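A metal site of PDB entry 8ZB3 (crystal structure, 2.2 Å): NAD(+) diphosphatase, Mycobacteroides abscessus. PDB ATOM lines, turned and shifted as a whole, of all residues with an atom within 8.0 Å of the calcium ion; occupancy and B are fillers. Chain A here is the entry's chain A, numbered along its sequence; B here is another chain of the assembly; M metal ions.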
ATOM      1  N   ALA A  19     -10.151 -11.195  32.208  1.00  0.00           N
ATOM      2  CA  ALA A  19      -9.854 -11.984  33.397  1.00  0.00           C
ATOM      3  C   ALA A  19     -10.535 -13.362  33.313  1.00  0.00           C
ATOM      4  O   ALA A  19     -11.280 -13.729  34.228  1.00  0.00           O
ATOM      5  CB  ALA A  19     -10.285 -11.226  34.632  1.00  0.00           C
ATOM      6  N   ASP A  20     -10.245 -14.080  32.237  1.00  0.00           N
ATOM      7  CA  ASP A  20     -10.958 -15.311  31.897  1.00  0.00           C
ATOM      8  C   ASP A  20     -10.870 -16.296  33.056  1.00  0.00           C
ATOM      9  O   ASP A  20     -11.868 -16.953  33.382  1.00  0.00           O
ATOM     10  CB  ASP A  20     -10.405 -15.898  30.597  1.00  0.00           C
ATOM     11  CG  ASP A  20      -8.995 -16.424  30.727  1.00  0.00           C
ATOM     12  OD1 ASP A  20      -8.040 -15.636  31.097  1.00  0.00           O
ATOM     13  OD2 ASP A  20      -8.828 -17.612  30.463  1.00  0.00           O
ATOM     14  N   GLU A  21      -9.717 -16.383  33.717  1.00  0.00           N
ATOM     15  CA  GLU A  21      -9.517 -17.407  34.746  1.00  0.00           C
ATOM     16  C   GLU A  21     -10.480 -17.203  35.914  1.00  0.00           C
ATOM     17  O   GLU A  21     -10.819 -18.199  36.573  1.00  0.00           O
ATOM     18  CB  GLU A  21      -8.062 -17.465  35.216  1.00  0.00           C
ATOM     19  CG  GLU A  21      -7.147 -18.035  34.149  1.00  0.00           C
ATOM     20  CD  GLU A  21      -7.591 -19.414  33.729  1.00  0.00           C
ATOM     21  OE1 GLU A  21      -7.920 -19.620  32.535  1.00  0.00           O
ATOM     22  OE2 GLU A  21      -7.696 -20.248  34.632  1.00  0.00           O
ATOM     23  N   LEU A  22     -10.959 -15.973  36.138  1.00  0.00           N
ATOM     24  CA  LEU A  22     -11.889 -15.749  37.233  1.00  0.00           C
ATOM     25  C   LEU A  22     -13.301 -16.245  36.942  1.00  0.00           C
ATOM     26  O   LEU A  22     -14.066 -16.489  37.902  1.00  0.00           O
ATOM     27  CB  LEU A  22     -11.953 -14.253  37.574  1.00  0.00           C
ATOM     28  CG  LEU A  22     -10.688 -13.669  38.206  1.00  0.00           C
ATOM     29  CD1 LEU A  22     -10.869 -12.205  38.547  1.00  0.00           C
ATOM     30  CD2 LEU A  22     -10.368 -14.468  39.466  1.00  0.00           C
ATOM     31  N   ARG A  23     -13.641 -16.437  35.663  1.00  0.00           N
ATOM     32  CA  ARG A  23     -14.960 -16.912  35.296  1.00  0.00           C
ATOM     33  C   ARG A  23     -15.249 -18.275  35.911  1.00  0.00           C
ATOM     34  O   ARG A  23     -16.394 -18.546  36.299  1.00  0.00           O
ATOM     35  CB  ARG A  23     -15.107 -17.054  33.765  1.00  0.00           C
ATOM     36  CG  ARG A  23     -15.005 -15.747  32.977  1.00  0.00           C
ATOM     37  CD  ARG A  23     -14.739 -16.074  31.518  1.00  0.00           C
ATOM     38  NE  ARG A  23     -14.680 -14.880  30.702  1.00  0.00           N
ATOM     39  CZ  ARG A  23     -14.450 -14.861  29.388  1.00  0.00           C
ATOM     40  NH1 ARG A  23     -14.237 -15.995  28.736  1.00  0.00           N
ATOM     41  NH2 ARG A  23     -14.453 -13.716  28.733  1.00  0.00           N
ATOM     42  N   SER A  24     -14.217 -19.138  35.962  1.00  0.00           N
ATOM     43  CA  SER A  24     -14.323 -20.479  36.498  1.00  0.00           C
ATOM     44  C   SER A  24     -13.934 -20.549  37.975  1.00  0.00           C
ATOM     45  O   SER A  24     -13.734 -21.637  38.490  1.00  0.00           O
ATOM     46  CB  SER A  24     -13.461 -21.410  35.688  1.00  0.00           C
ATOM     47  OG  SER A  24     -13.880 -21.421  34.337  1.00  0.00           O
ATOM     48  N   ARG B 206      -5.465 -12.082  22.368  1.00  0.00           N
ATOM     49  CA  ARG B 206      -5.939 -12.610  23.644  1.00  0.00           C
ATOM     50  C   ARG B 206      -5.569 -14.101  23.750  1.00  0.00           C
ATOM     51  O   ARG B 206      -5.045 -14.535  24.761  1.00  0.00           O
ATOM     52  CB  ARG B 206      -7.441 -12.361  23.803  1.00  0.00           C
ATOM     53  CG  ARG B 206      -8.048 -12.961  25.052  1.00  0.00           C
ATOM     54  CD  ARG B 206      -9.561 -12.730  25.170  1.00  0.00           C
ATOM     55  NE  ARG B 206     -10.332 -13.299  24.065  1.00  0.00           N
ATOM     56  CZ  ARG B 206     -10.374 -14.588  23.744  1.00  0.00           C
ATOM     57  NH1 ARG B 206      -9.822 -15.503  24.512  1.00  0.00           N
ATOM     58  NH2 ARG B 206     -11.006 -14.999  22.651  1.00  0.00           N
ATOM     59  N   GLU B 207      -5.871 -14.868  22.694  1.00  0.00           N
ATOM     60  CA  GLU B 207      -5.693 -16.306  22.720  1.00  0.00           C
ATOM     61  C   GLU B 207      -4.209 -16.690  22.804  1.00  0.00           C
ATOM     62  O   GLU B 207      -3.848 -17.615  23.488  1.00  0.00           O
ATOM     63  CB  GLU B 207      -6.340 -16.962  21.508  1.00  0.00           C
ATOM     64  CG  GLU B 207      -7.858 -17.012  21.586  1.00  0.00           C
ATOM     65  CD  GLU B 207      -8.450 -18.001  22.581  1.00  0.00           C
ATOM     66  OE1 GLU B 207      -9.650 -17.948  22.796  1.00  0.00           O
ATOM     67  OE2 GLU B 207      -7.714 -18.792  23.164  1.00  0.00           O
ATOM     68  N   ALA B 209      -1.881 -14.907  24.224  1.00  0.00           N
ATOM     69  CA  ALA B 209      -1.530 -14.589  25.602  1.00  0.00           C
ATOM     70  C   ALA B 209      -2.022 -15.693  26.557  1.00  0.00           C
ATOM     71  O   ALA B 209      -1.254 -16.140  27.396  1.00  0.00           O
ATOM     72  CB  ALA B 209      -2.070 -13.225  25.998  1.00  0.00           C
ATOM     73  N   GLU B 210      -3.277 -16.125  26.391  1.00  0.00           N
ATOM     74  CA  GLU B 210      -3.862 -17.161  27.233  1.00  0.00           C
ATOM     75  C   GLU B 210      -3.073 -18.473  27.128  1.00  0.00           C
ATOM     76  O   GLU B 210      -2.919 -19.175  28.113  1.00  0.00           O
ATOM     77  CB  GLU B 210      -5.298 -17.489  26.834  1.00  0.00           C
ATOM     78  CG  GLU B 210      -6.311 -16.468  27.298  1.00  0.00           C
ATOM     79  CD  GLU B 210      -6.348 -16.321  28.808  1.00  0.00           C
ATOM     80  OE1 GLU B 210      -6.395 -17.366  29.501  1.00  0.00           O
ATOM     81  OE2 GLU B 210      -6.309 -15.165  29.292  1.00  0.00           O
ATOM     82  N   GLU B 211      -2.599 -18.829  25.932  1.00  0.00           N
ATOM     83  CA  GLU B 211      -2.079 -20.151  25.704  1.00  0.00           C
ATOM     84  C   GLU B 211      -0.592 -20.234  26.047  1.00  0.00           C
ATOM     85  O   GLU B 211      -0.134 -21.212  26.638  1.00  0.00           O
ATOM     86  CB  GLU B 211      -2.285 -20.589  24.256  1.00  0.00           C
ATOM     87  CG  GLU B 211      -3.768 -20.666  23.873  1.00  0.00           C
ATOM     88  CD  GLU B 211      -4.544 -21.780  24.571  1.00  0.00           C
ATOM     89  OE1 GLU B 211      -5.527 -21.453  25.286  1.00  0.00           O
ATOM     90  OE2 GLU B 211      -4.187 -22.957  24.391  1.00  0.00           O
ATOM     91  N   PHE B 249       2.253 -20.964  30.611  1.00  0.00           N
ATOM     92  CA  PHE B 249       1.235 -21.867  30.115  1.00  0.00           C
ATOM     93  C   PHE B 249       0.054 -21.989  31.049  1.00  0.00           C
ATOM     94  O   PHE B 249      -0.830 -22.760  30.703  1.00  0.00           O
ATOM     95  CB  PHE B 249       1.842 -23.250  29.944  1.00  0.00           C
ATOM     96  CG  PHE B 249       3.026 -23.255  29.018  1.00  0.00           C
ATOM     97  CD1 PHE B 249       2.939 -22.657  27.768  1.00  0.00           C
ATOM     98  CD2 PHE B 249       4.215 -23.831  29.415  1.00  0.00           C
ATOM     99  CE1 PHE B 249       4.033 -22.670  26.924  1.00  0.00           C
ATOM    100  CE2 PHE B 249       5.305 -23.856  28.565  1.00  0.00           C
ATOM    101  CZ  PHE B 249       5.222 -23.267  27.329  1.00  0.00           C
ATOM    102  N   ASN B 250       0.054 -21.310  32.200  1.00  0.00           N
ATOM    103  CA  ASN B 250      -0.930 -21.621  33.236  1.00  0.00           C
ATOM    104  C   ASN B 250      -2.355 -21.296  32.771  1.00  0.00           C
ATOM    105  O   ASN B 250      -3.175 -22.185  32.876  1.00  0.00           O
ATOM    106  CB  ASN B 250      -0.543 -21.128  34.638  1.00  0.00           C
ATOM    107  CG  ASN B 250      -0.170 -19.672  34.723  1.00  0.00           C
ATOM    108  OD1 ASN B 250       0.743 -19.234  34.023  1.00  0.00           O
ATOM    109  ND2 ASN B 250      -0.859 -18.931  35.587  1.00  0.00           N
ATOM    110  N   ASP B 251      -2.584 -20.127  32.145  1.00  0.00           N
ATOM    111  CA  ASP B 251      -3.925 -19.680  31.811  1.00  0.00           C
ATOM    112  C   ASP B 251      -4.542 -20.493  30.650  1.00  0.00           C
ATOM    113  O   ASP B 251      -5.695 -20.284  30.343  1.00  0.00           O
ATOM    114  CB  ASP B 251      -3.907 -18.192  31.470  1.00  0.00           C
ATOM    115  CG  ASP B 251      -3.953 -17.240  32.657  1.00  0.00           C
ATOM    116  OD1 ASP B 251      -3.426 -17.606  33.741  1.00  0.00           O
ATOM    117  OD2 ASP B 251      -4.513 -16.121  32.487  1.00  0.00           O
ATOM    118  N   GLY B 252      -3.800 -21.397  30.013  1.00  0.00           N
ATOM    119  CA  GLY B 252      -4.226 -22.005  28.761  1.00  0.00           C
ATOM    120  C   GLY B 252      -4.290 -23.522  28.801  1.00  0.00           C
ATOM    121  O   GLY B 252      -4.234 -24.106  29.882  1.00  0.00           O
ATOM    122  N   GLU B 253      -4.335 -24.145  27.627  1.00  0.00           N
ATOM    123  CA  GLU B 253      -4.413 -25.590  27.487  1.00  0.00           C
ATOM    124  C   GLU B 253      -3.130 -26.121  26.864  1.00  0.00           C
ATOM    125  O   GLU B 253      -3.164 -27.204  26.297  1.00  0.00           O
ATOM    126  CB  GLU B 253      -5.614 -25.999  26.623  1.00  0.00           C
ATOM    127  CG  GLU B 253      -6.866 -26.334  27.451  1.00  0.00           C
ATOM    128  CD  GLU B 253      -7.592 -25.118  27.998  1.00  0.00           C
ATOM    129  OE1 GLU B 253      -7.946 -24.260  27.168  1.00  0.00           O
ATOM    130  OE2 GLU B 253      -7.771 -25.003  29.232  1.00  0.00           O
HETATM  131 CA    CA M   1      -7.567 -19.088  30.420  1.00  0.00          CA
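The side-chain amide nitrogen (ND2) of Asn 250 of chain B sits at hydrogen-bond distance from the side-chain carboxylate (OD1) of Asp 251 of chain B (3.4 Å).
O of Glu 210 of chain B is in hydrogen-bond range of N of Gly 252 of chain B.
Of the 16 residues printed, 4 come within 4 Å of the calcium ion.
Along chain A the residues within 4 Å of the calcium ion span positions 20 to 21.
The calcium ion is bound by the side-chain carboxylate (OD2) of Asp 20 (1.9 Å), the side-chain carboxylate (OE1) of Glu 21 (2.2 Å), the backbone carbonyl oxygen (O) of Asp 251 of chain B (2.2 Å) and the side-chain carboxylate (OE1) of Glu 210 of chain B (2.3 Å).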
